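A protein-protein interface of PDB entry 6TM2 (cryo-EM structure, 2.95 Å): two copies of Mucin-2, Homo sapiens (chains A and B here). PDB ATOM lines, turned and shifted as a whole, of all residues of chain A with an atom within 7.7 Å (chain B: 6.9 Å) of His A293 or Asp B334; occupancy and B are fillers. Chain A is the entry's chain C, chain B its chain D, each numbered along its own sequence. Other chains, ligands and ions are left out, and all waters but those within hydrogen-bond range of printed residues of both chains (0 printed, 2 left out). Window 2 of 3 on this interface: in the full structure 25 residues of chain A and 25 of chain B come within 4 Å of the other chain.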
ATOM      1  N   PRO A 287      27.810   6.676 -18.631  1.00  0.00           N
ATOM      2  CA  PRO A 287      27.209   6.370 -19.931  1.00  0.00           C
ATOM      3  C   PRO A 287      25.875   7.037 -20.175  1.00  0.00           C
ATOM      4  O   PRO A 287      25.585   7.391 -21.319  1.00  0.00           O
ATOM      5  CB  PRO A 287      27.064   4.847 -19.884  1.00  0.00           C
ATOM      6  CG  PRO A 287      28.042   4.409 -18.923  1.00  0.00           C
ATOM      7  CD  PRO A 287      28.069   5.451 -17.872  1.00  0.00           C
ATOM      8  N   CYS A 288      25.044   7.211 -19.153  1.00  0.00           N
ATOM      9  CA  CYS A 288      23.744   7.826 -19.364  1.00  0.00           C
ATOM     10  C   CYS A 288      23.823   9.342 -19.454  1.00  0.00           C
ATOM     11  O   CYS A 288      22.807   9.985 -19.729  1.00  0.00           O
ATOM     12  CB  CYS A 288      22.772   7.418 -18.255  1.00  0.00           C
ATOM     13  SG  CYS A 288      22.350   5.645 -18.134  1.00  0.00           S
ATOM     14  N   SER A 289      25.003   9.920 -19.229  1.00  0.00           N
ATOM     15  CA  SER A 289      25.285  11.322 -19.495  1.00  0.00           C
ATOM     16  C   SER A 289      25.940  11.542 -20.844  1.00  0.00           C
ATOM     17  O   SER A 289      25.730  12.588 -21.458  1.00  0.00           O
ATOM     18  CB  SER A 289      26.195  11.890 -18.406  1.00  0.00           C
ATOM     19  OG  SER A 289      25.544  11.855 -17.152  1.00  0.00           O
ATOM     20  N   LEU A 290      26.722  10.579 -21.317  1.00  0.00           N
ATOM     21  CA  LEU A 290      27.284  10.626 -22.656  1.00  0.00           C
ATOM     22  C   LEU A 290      26.313  10.141 -23.719  1.00  0.00           C
ATOM     23  O   LEU A 290      26.571  10.348 -24.908  1.00  0.00           O
ATOM     24  CB  LEU A 290      28.561   9.793 -22.710  1.00  0.00           C
ATOM     25  CG  LEU A 290      29.708  10.322 -21.854  1.00  0.00           C
ATOM     26  CD1 LEU A 290      30.860   9.362 -21.855  1.00  0.00           C
ATOM     27  CD2 LEU A 290      30.149  11.670 -22.357  1.00  0.00           C
ATOM     28  N   ASN A 291      25.223   9.486 -23.322  1.00  0.00           N
ATOM     29  CA  ASN A 291      24.142   9.078 -24.221  1.00  0.00           C
ATOM     30  C   ASN A 291      22.825   9.510 -23.598  1.00  0.00           C
ATOM     31  O   ASN A 291      22.161   8.709 -22.933  1.00  0.00           O
ATOM     32  CB  ASN A 291      24.136   7.569 -24.453  1.00  0.00           C
ATOM     33  CG  ASN A 291      25.302   7.092 -25.272  1.00  0.00           C
ATOM     34  OD1 ASN A 291      25.677   7.708 -26.261  1.00  0.00           O
ATOM     35  ND2 ASN A 291      25.884   5.980 -24.865  1.00  0.00           N
ATOM     36  N   PRO A 292      22.420  10.773 -23.780  1.00  0.00           N
ATOM     37  CA  PRO A 292      21.166  11.233 -23.163  1.00  0.00           C
ATOM     38  C   PRO A 292      19.926  10.633 -23.792  1.00  0.00           C
ATOM     39  O   PRO A 292      18.887  10.555 -23.132  1.00  0.00           O
ATOM     40  CB  PRO A 292      21.208  12.747 -23.383  1.00  0.00           C
ATOM     41  CG  PRO A 292      22.616  13.064 -23.615  1.00  0.00           C
ATOM     42  CD  PRO A 292      23.179  11.901 -24.340  1.00  0.00           C
ATOM     43  N   HIS A 293      20.012  10.201 -25.040  1.00  0.00           N
ATOM     44  CA  HIS A 293      18.888   9.663 -25.785  1.00  0.00           C
ATOM     45  C   HIS A 293      18.589   8.210 -25.459  1.00  0.00           C
ATOM     46  O   HIS A 293      17.519   7.722 -25.823  1.00  0.00           O
ATOM     47  CB  HIS A 293      19.164   9.846 -27.276  1.00  0.00           C
ATOM     48  CG  HIS A 293      20.406   9.157 -27.753  1.00  0.00           C
ATOM     49  ND1 HIS A 293      21.667   9.666 -27.529  1.00  0.00           N
ATOM     50  CD2 HIS A 293      20.583   8.027 -28.477  1.00  0.00           C
ATOM     51  CE1 HIS A 293      22.566   8.863 -28.063  1.00  0.00           C
ATOM     52  NE2 HIS A 293      21.935   7.863 -28.649  1.00  0.00           N
ATOM     53  N   ARG A 294      19.485   7.517 -24.767  1.00  0.00           N
ATOM     54  CA  ARG A 294      19.286   6.127 -24.386  1.00  0.00           C
ATOM     55  C   ARG A 294      18.821   5.957 -22.947  1.00  0.00           C
ATOM     56  O   ARG A 294      18.587   4.826 -22.521  1.00  0.00           O
ATOM     57  CB  ARG A 294      20.571   5.344 -24.608  1.00  0.00           C
ATOM     58  CG  ARG A 294      20.924   5.210 -26.052  1.00  0.00           C
ATOM     59  CD  ARG A 294      22.190   4.433 -26.234  1.00  0.00           C
ATOM     60  NE  ARG A 294      22.029   3.078 -25.735  1.00  0.00           N
ATOM     61  CZ  ARG A 294      21.544   2.057 -26.426  1.00  0.00           C
ATOM     62  NH1 ARG A 294      21.156   2.205 -27.676  1.00  0.00           N
ATOM     63  NH2 ARG A 294      21.443   0.878 -25.851  1.00  0.00           N
ATOM     64  N   ARG A 295      18.662   7.054 -22.205  1.00  0.00           N
ATOM     65  CA  ARG A 295      18.293   6.998 -20.795  1.00  0.00           C
ATOM     66  C   ARG A 295      16.831   6.629 -20.597  1.00  0.00           C
ATOM     67  O   ARG A 295      16.496   5.941 -19.630  1.00  0.00           O
ATOM     68  CB  ARG A 295      18.573   8.346 -20.142  1.00  0.00           C
ATOM     69  CG  ARG A 295      18.261   8.430 -18.664  1.00  0.00           C
ATOM     70  CD  ARG A 295      18.532   9.799 -18.129  1.00  0.00           C
ATOM     71  NE  ARG A 295      19.952  10.102 -18.105  1.00  0.00           N
ATOM     72  CZ  ARG A 295      20.445  11.315 -17.893  1.00  0.00           C
ATOM     73  NH1 ARG A 295      19.628  12.340 -17.710  1.00  0.00           N
ATOM     74  NH2 ARG A 295      21.753  11.510 -17.885  1.00  0.00           N
ATOM     75  N   SER A 296      15.947   7.077 -21.481  1.00  0.00           N
ATOM     76  CA  SER A 296      14.520   6.855 -21.275  1.00  0.00           C
ATOM     77  C   SER A 296      14.140   5.405 -21.519  1.00  0.00           C
ATOM     78  O   SER A 296      13.237   4.879 -20.865  1.00  0.00           O
ATOM     79  CB  SER A 296      13.721   7.773 -22.187  1.00  0.00           C
ATOM     80  OG  SER A 296      13.974   9.123 -21.866  1.00  0.00           O
ATOM     81  N   TRP A 297      14.805   4.751 -22.468  1.00  0.00           N
ATOM     82  CA  TRP A 297      14.586   3.329 -22.684  1.00  0.00           C
ATOM     83  C   TRP A 297      15.155   2.511 -21.541  1.00  0.00           C
ATOM     84  O   TRP A 297      14.534   1.542 -21.102  1.00  0.00           O
ATOM     85  CB  TRP A 297      15.230   2.889 -23.990  1.00  0.00           C
ATOM     86  CG  TRP A 297      15.030   1.445 -24.283  1.00  0.00           C
ATOM     87  CD1 TRP A 297      13.873   0.842 -24.637  1.00  0.00           C
ATOM     88  CD2 TRP A 297      16.007   0.406 -24.173  1.00  0.00           C
ATOM     89  NE1 TRP A 297      14.068  -0.497 -24.800  1.00  0.00           N
ATOM     90  CE2 TRP A 297      15.372  -0.793 -24.516  1.00  0.00           C
ATOM     91  CE3 TRP A 297      17.365   0.381 -23.843  1.00  0.00           C
ATOM     92  CZ2 TRP A 297      16.038  -2.010 -24.525  1.00  0.00           C
ATOM     93  CZ3 TRP A 297      18.021  -0.822 -23.847  1.00  0.00           C
ATOM     94  CH2 TRP A 297      17.360  -2.004 -24.188  1.00  0.00           C
ATOM     95  N   ALA A 298      16.345   2.877 -21.070  1.00  0.00           N
ATOM     96  CA  ALA A 298      17.049   2.081 -20.074  1.00  0.00           C
ATOM     97  C   ALA A 298      16.332   2.098 -18.737  1.00  0.00           C
ATOM     98  O   ALA A 298      16.200   1.061 -18.089  1.00  0.00           O
ATOM     99  CB  ALA A 298      18.473   2.589 -19.911  1.00  0.00           C
ATOM    100  N   CYS A 331      22.558   2.041 -21.166  1.00  0.00           N
ATOM    101  CA  CYS A 331      22.939   3.294 -21.800  1.00  0.00           C
ATOM    102  C   CYS A 331      24.232   3.192 -22.591  1.00  0.00           C
ATOM    103  O   CYS A 331      24.544   4.115 -23.344  1.00  0.00           O
ATOM    104  CB  CYS A 331      23.100   4.407 -20.770  1.00  0.00           C
ATOM    105  SG  CYS A 331      21.640   5.014 -19.937  1.00  0.00           S
ATOM    106  N   CYS A 333      25.473   0.161 -24.397  1.00  0.00           N
ATOM    107  CA  CYS A 333      25.577  -0.803 -25.491  1.00  0.00           C
ATOM    108  C   CYS A 333      25.078  -0.164 -26.786  1.00  0.00           C
ATOM    109  O   CYS A 333      24.089  -0.573 -27.391  1.00  0.00           O
ATOM    110  CB  CYS A 333      24.826  -2.088 -25.147  1.00  0.00           C
ATOM    111  SG  CYS A 333      25.592  -2.989 -23.760  1.00  0.00           S
ATOM    112  N   ASP A 334      25.812   0.861 -27.213  1.00  0.00           N
ATOM    113  CA  ASP A 334      25.386   1.752 -28.280  1.00  0.00           C
ATOM    114  C   ASP A 334      25.985   1.418 -29.639  1.00  0.00           C
ATOM    115  O   ASP A 334      25.825   2.197 -30.577  1.00  0.00           O
ATOM    116  CB  ASP A 334      25.691   3.205 -27.898  1.00  0.00           C
ATOM    117  CG  ASP A 334      27.155   3.460 -27.610  1.00  0.00           C
ATOM    118  OD1 ASP A 334      27.960   2.519 -27.595  1.00  0.00           O
ATOM    119  OD2 ASP A 334      27.515   4.626 -27.405  1.00  0.00           O
ATOM    120  N   ASP A 338      21.741  -4.516 -27.720  1.00  0.00           N
ATOM    121  CA  ASP A 338      21.562  -3.996 -26.377  1.00  0.00           C
ATOM    122  C   ASP A 338      20.527  -4.761 -25.577  1.00  0.00           C
ATOM    123  O   ASP A 338      20.459  -4.588 -24.358  1.00  0.00           O
ATOM    124  CB  ASP A 338      21.206  -2.499 -26.422  1.00  0.00           C
ATOM    125  CG  ASP A 338      19.923  -2.194 -27.183  1.00  0.00           C
ATOM    126  OD1 ASP A 338      19.283  -3.089 -27.742  1.00  0.00           O
ATOM    127  OD2 ASP A 338      19.544  -1.015 -27.223  1.00  0.00           O
ATOM    128  N   CYS B 160      11.104   6.883 -35.047  1.00  0.00           N
ATOM    129  CA  CYS B 160      11.713   5.840 -34.232  1.00  0.00           C
ATOM    130  C   CYS B 160      13.220   5.879 -34.461  1.00  0.00           C
ATOM    131  O   CYS B 160      13.745   5.303 -35.414  1.00  0.00           O
ATOM    132  CB  CYS B 160      11.073   4.469 -34.510  1.00  0.00           C
ATOM    133  SG  CYS B 160      11.063   3.818 -36.193  1.00  0.00           S
ATOM    134  N   GLY B 161      13.913   6.588 -33.573  1.00  0.00           N
ATOM    135  CA  GLY B 161      15.332   6.849 -33.623  1.00  0.00           C
ATOM    136  C   GLY B 161      15.603   8.319 -33.415  1.00  0.00           C
ATOM    137  O   GLY B 161      14.739   9.079 -32.968  1.00  0.00           O
ATOM    138  N   THR B 162      16.828   8.734 -33.730  1.00  0.00           N
ATOM    139  CA  THR B 162      17.210  10.139 -33.700  1.00  0.00           C
ATOM    140  C   THR B 162      17.673  10.668 -35.047  1.00  0.00           C
ATOM    141  O   THR B 162      17.960  11.862 -35.155  1.00  0.00           O
ATOM    142  CB  THR B 162      18.320  10.391 -32.670  1.00  0.00           C
ATOM    143  OG1 THR B 162      19.485   9.641 -33.019  1.00  0.00           O
ATOM    144  CG2 THR B 162      17.881  10.009 -31.280  1.00  0.00           C
ATOM    145  N   THR B 163      17.735   9.830 -36.076  1.00  0.00           N
ATOM    146  CA  THR B 163      18.269  10.213 -37.375  1.00  0.00           C
ATOM    147  C   THR B 163      17.244  10.840 -38.307  1.00  0.00           C
ATOM    148  O   THR B 163      17.632  11.364 -39.352  1.00  0.00           O
ATOM    149  CB  THR B 163      18.889   8.997 -38.067  1.00  0.00           C
ATOM    150  OG1 THR B 163      17.905   7.973 -38.195  1.00  0.00           O
ATOM    151  CG2 THR B 163      20.049   8.460 -37.273  1.00  0.00           C
ATOM    152  N   LEU B 290      24.785   8.773 -40.531  1.00  0.00           N
ATOM    153  CA  LEU B 290      24.604   9.534 -39.306  1.00  0.00           C
ATOM    154  C   LEU B 290      24.974   8.743 -38.063  1.00  0.00           C
ATOM    155  O   LEU B 290      25.093   9.336 -36.987  1.00  0.00           O
ATOM    156  CB  LEU B 290      23.157  10.006 -39.201  1.00  0.00           C
ATOM    157  CG  LEU B 290      22.730  11.004 -40.273  1.00  0.00           C
ATOM    158  CD1 LEU B 290      21.262  11.293 -40.178  1.00  0.00           C
ATOM    159  CD2 LEU B 290      23.523  12.277 -40.141  1.00  0.00           C
ATOM    160  N   ASN B 291      25.134   7.426 -38.181  1.00  0.00           N
ATOM    161  CA  ASN B 291      25.616   6.561 -37.102  1.00  0.00           C
ATOM    162  C   ASN B 291      26.723   5.684 -37.662  1.00  0.00           C
ATOM    163  O   ASN B 291      26.470   4.540 -38.051  1.00  0.00           O
ATOM    164  CB  ASN B 291      24.500   5.689 -36.533  1.00  0.00           C
ATOM    165  CG  ASN B 291      23.477   6.469 -35.757  1.00  0.00           C
ATOM    166  OD1 ASN B 291      23.809   7.355 -34.980  1.00  0.00           O
ATOM    167  ND2 ASN B 291      22.215   6.139 -35.960  1.00  0.00           N
ATOM    168  N   HIS B 293      29.208   4.299 -36.121  1.00  0.00           N
ATOM    169  CA  HIS B 293      29.603   3.288 -35.158  1.00  0.00           C
ATOM    170  C   HIS B 293      28.657   2.100 -35.110  1.00  0.00           C
ATOM    171  O   HIS B 293      29.014   1.073 -34.532  1.00  0.00           O
ATOM    172  CB  HIS B 293      29.724   3.949 -33.786  1.00  0.00           C
ATOM    173  CG  HIS B 293      28.455   4.579 -33.301  1.00  0.00           C
ATOM    174  ND1 HIS B 293      28.007   5.796 -33.768  1.00  0.00           N
ATOM    175  CD2 HIS B 293      27.562   4.189 -32.361  1.00  0.00           C
ATOM    176  CE1 HIS B 293      26.877   6.109 -33.165  1.00  0.00           C
ATOM    177  NE2 HIS B 293      26.587   5.153 -32.302  1.00  0.00           N
ATOM    178  N   ARG B 294      27.481   2.199 -35.718  1.00  0.00           N
ATOM    179  CA  ARG B 294      26.514   1.114 -35.749  1.00  0.00           C
ATOM    180  C   ARG B 294      26.529   0.329 -37.053  1.00  0.00           C
ATOM    181  O   ARG B 294      25.776  -0.636 -37.182  1.00  0.00           O
ATOM    182  CB  ARG B 294      25.118   1.662 -35.493  1.00  0.00           C
ATOM    183  CG  ARG B 294      24.944   2.177 -34.103  1.00  0.00           C
ATOM    184  CD  ARG B 294      23.561   2.704 -33.886  1.00  0.00           C
ATOM    185  NE  ARG B 294      22.583   1.641 -34.043  1.00  0.00           N
ATOM    186  CZ  ARG B 294      22.194   0.808 -33.089  1.00  0.00           C
ATOM    187  NH1 ARG B 294      22.689   0.889 -31.872  1.00  0.00           N
ATOM    188  NH2 ARG B 294      21.303  -0.119 -33.367  1.00  0.00           N
ATOM    189  N   ASP B 329      17.646  -0.522 -41.190  1.00  0.00           N
ATOM    190  CA  ASP B 329      16.843  -0.583 -39.974  1.00  0.00           C
ATOM    191  C   ASP B 329      17.683  -0.700 -38.718  1.00  0.00           C
ATOM    192  O   ASP B 329      17.270  -0.218 -37.663  1.00  0.00           O
ATOM    193  CB  ASP B 329      15.865  -1.755 -40.014  1.00  0.00           C
ATOM    194  CG  ASP B 329      14.734  -1.546 -40.985  1.00  0.00           C
ATOM    195  OD1 ASP B 329      14.376  -0.390 -41.250  1.00  0.00           O
ATOM    196  OD2 ASP B 329      14.181  -2.548 -41.478  1.00  0.00           O
ATOM    197  N   SER B 330      18.843  -1.338 -38.794  1.00  0.00           N
ATOM    198  CA  SER B 330      19.656  -1.587 -37.616  1.00  0.00           C
ATOM    199  C   SER B 330      20.615  -0.457 -37.305  1.00  0.00           C
ATOM    200  O   SER B 330      21.045  -0.332 -36.157  1.00  0.00           O
ATOM    201  CB  SER B 330      20.440  -2.883 -37.787  1.00  0.00           C
ATOM    202  OG  SER B 330      19.565  -3.981 -37.915  1.00  0.00           O
ATOM    203  N   CYS B 331      20.965   0.369 -38.285  1.00  0.00           N
ATOM    204  CA  CYS B 331      21.740   1.568 -37.998  1.00  0.00           C
ATOM    205  C   CYS B 331      20.917   2.667 -37.348  1.00  0.00           C
ATOM    206  O   CYS B 331      21.497   3.638 -36.863  1.00  0.00           O
ATOM    207  CB  CYS B 331      22.370   2.134 -39.266  1.00  0.00           C
ATOM    208  SG  CYS B 331      23.679   1.206 -40.054  1.00  0.00           S
ATOM    209  N   SER B 332      19.598   2.542 -37.299  1.00  0.00           N
ATOM    210  CA  SER B 332      18.749   3.637 -36.876  1.00  0.00           C
ATOM    211  C   SER B 332      17.915   3.352 -35.640  1.00  0.00           C
ATOM    212  O   SER B 332      17.164   4.232 -35.215  1.00  0.00           O
ATOM    213  CB  SER B 332      17.825   4.047 -38.024  1.00  0.00           C
ATOM    214  OG  SER B 332      16.938   3.010 -38.372  1.00  0.00           O
ATOM    215  N   CYS B 333      18.013   2.170 -35.043  1.00  0.00           N
ATOM    216  CA  CYS B 333      17.333   1.910 -33.776  1.00  0.00           C
ATOM    217  C   CYS B 333      18.277   2.217 -32.614  1.00  0.00           C
ATOM    218  O   CYS B 333      18.666   1.354 -31.830  1.00  0.00           O
ATOM    219  CB  CYS B 333      16.803   0.478 -33.736  1.00  0.00           C
ATOM    220  SG  CYS B 333      15.478   0.193 -34.954  1.00  0.00           S
ATOM    221  N   ASP B 334      18.629   3.496 -32.514  1.00  0.00           N
ATOM    222  CA  ASP B 334      19.693   3.960 -31.638  1.00  0.00           C
ATOM    223  C   ASP B 334      19.201   4.520 -30.311  1.00  0.00           C
ATOM    224  O   ASP B 334      19.996   5.087 -29.564  1.00  0.00           O
ATOM    225  CB  ASP B 334      20.559   4.990 -32.372  1.00  0.00           C
ATOM    226  CG  ASP B 334      19.781   6.191 -32.866  1.00  0.00           C
ATOM    227  OD1 ASP B 334      18.548   6.224 -32.752  1.00  0.00           O
ATOM    228  OD2 ASP B 334      20.413   7.130 -33.368  1.00  0.00           O
ATOM    229  N   THR B 335      17.922   4.373 -29.993  1.00  0.00           N
ATOM    230  CA  THR B 335      17.423   4.788 -28.695  1.00  0.00           C
ATOM    231  C   THR B 335      17.089   3.619 -27.787  1.00  0.00           C
ATOM    232  O   THR B 335      17.010   3.810 -26.575  1.00  0.00           O
ATOM    233  CB  THR B 335      16.179   5.673 -28.850  1.00  0.00           C
ATOM    234  OG1 THR B 335      15.142   4.931 -29.496  1.00  0.00           O
ATOM    235  CG2 THR B 335      16.495   6.895 -29.673  1.00  0.00           C
ATOM    236  N   GLY B 336      16.905   2.425 -28.334  1.00  0.00           N
ATOM    237  CA  GLY B 336      16.715   1.247 -27.522  1.00  0.00           C
ATOM    238  C   GLY B 336      15.974   0.132 -28.218  1.00  0.00           C
ATOM    239  O   GLY B 336      15.042   0.380 -28.981  1.00  0.00           O
ATOM    240  N   GLY B 337      16.381  -1.105 -27.961  1.00  0.00           N
ATOM    241  CA  GLY B 337      15.719  -2.264 -28.520  1.00  0.00           C
ATOM    242  C   GLY B 337      15.972  -2.482 -29.994  1.00  0.00           C
ATOM    243  O   GLY B 337      15.049  -2.404 -30.805  1.00  0.00           O
ATOM    244  N   ASP B 338      17.218  -2.759 -30.361  1.00  0.00           N
ATOM    245  CA  ASP B 338      17.584  -2.883 -31.760  1.00  0.00           C
ATOM    246  C   ASP B 338      17.582  -4.317 -32.249  1.00  0.00           C
ATOM    247  O   ASP B 338      17.627  -4.541 -33.461  1.00  0.00           O
ATOM    248  CB  ASP B 338      18.954  -2.230 -32.019  1.00  0.00           C
ATOM    249  CG  ASP B 338      20.091  -2.844 -31.215  1.00  0.00           C
ATOM    250  OD1 ASP B 338      19.882  -3.748 -30.401  1.00  0.00           O
ATOM    251  OD2 ASP B 338      21.233  -2.402 -31.404  1.00  0.00           O
ATOM    252  N   CYS B 341      14.301  -4.641 -34.108  1.00  0.00           N
ATOM    253  CA  CYS B 341      14.380  -4.090 -35.451  1.00  0.00           C
ATOM    254  C   CYS B 341      15.082  -5.050 -36.396  1.00  0.00           C
ATOM    255  O   CYS B 341      14.830  -5.028 -37.602  1.00  0.00           O
ATOM    256  CB  CYS B 341      15.142  -2.768 -35.422  1.00  0.00           C
ATOM    257  SG  CYS B 341      14.452  -1.466 -34.385  1.00  0.00           S
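The side-chain carboxylate (OD2) of Asp A338 lies within hydrogen-bond range of the backbone NH (N) of Gly B337 (3.2 Å). N of Asp A338 sits at hydrogen-bond distance from OD1 of Asp B338 (3.4 Å).
OD2 of Asp A334 is in hydrogen-bond range of ND2 of Asn A291 (3.3 Å). The guanidinium group (NH2) of Arg B294 sits at hydrogen-bond distance from the backbone carbonyl oxygen (O) of Ser B330 (2.8 Å). NH2 of Arg B294 is in hydrogen-bond range of O of Cys B333. The guanidinium group (NH2) of Arg B294 is in salt-bridge range of the side-chain carboxylate (OD2) of Asp B338 (3.0 Å). The side-chain sulfur (SG) of Cys A288 forms a disulfide with the side-chain sulfur (SG) of Cys A331, at 2.0 Å. SG of Cys B341 is disulfide-bonded to SG of Cys B333 (2.0 Å).
Among the printed residues, pairs that only touch across the chains: Asp A334 with His B293 (3.2 Å), His A293 with Asp B334 (3.2 Å), Trp A297 with Thr B335 (3.3 Å), Trp A297 with Gly B336 (3.5 Å), Trp A297 with Gly B337 (3.6 Å), Asp A334 with Arg B294 (3.6 Å), Asp A338 with Gly B336 (3.6 Å), Arg A294 with Asp B334 (3.6 Å), His A293 with Thr B335 (3.9 Å) and Arg A294 with Thr B335 (3.9 Å).
Ser A289 touches none of the printed residues of chain B. Of chain B, only Asp B334 and Thr B335 come within 4 Å of His A293. Of the printed residues of chain B, Trp A297 touches Thr B335 (3.3 Å), Gly B336 (3.5 Å) and Gly B337 (3.6 Å). Of the printed residues of chain B, Asp A338 touches Gly B336 (3.6 Å), Gly B337 (3.2 Å) and Asp B338 (2.8 Å). Of chain A, only His A293 and Arg A294 come within 4 Å of Asp B334. Printed residues of chain A within 4 Å of Gly B337: Trp A297 (3.6 Å) and Asp A338 (3.2 Å). Cys B341 touches none of the printed residues of chain A. The nearest residue of chain B that does not touch His A293 is Thr B162 (4.2 Å). The nearest residue of chain A that does not touch Asp B334 is Asp A334 (6.2 Å).
Hydrophobic or aromatic side chains of chain B that line the printed part of chain A: His B293. Of the 16 printed residues of chain A, 5 touch a printed residue of chain B. Among the printed residues, no Asp or Glu carboxylate lies within 4 Å of a Lys or Arg side-chain nitrogen of the other chain.
His A293 touches Asp B334, and with the chains exchanged Asp A334 touches His B293. Arg A294 touches Asp B334, and with the chains exchanged Asp A334 touches Arg B294. Asp B338 touches its own counterpart, Asp A338. Of the 12 pairs that touch across the chains among the printed residues, 5 have their exchanged pair printed and touching as well.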
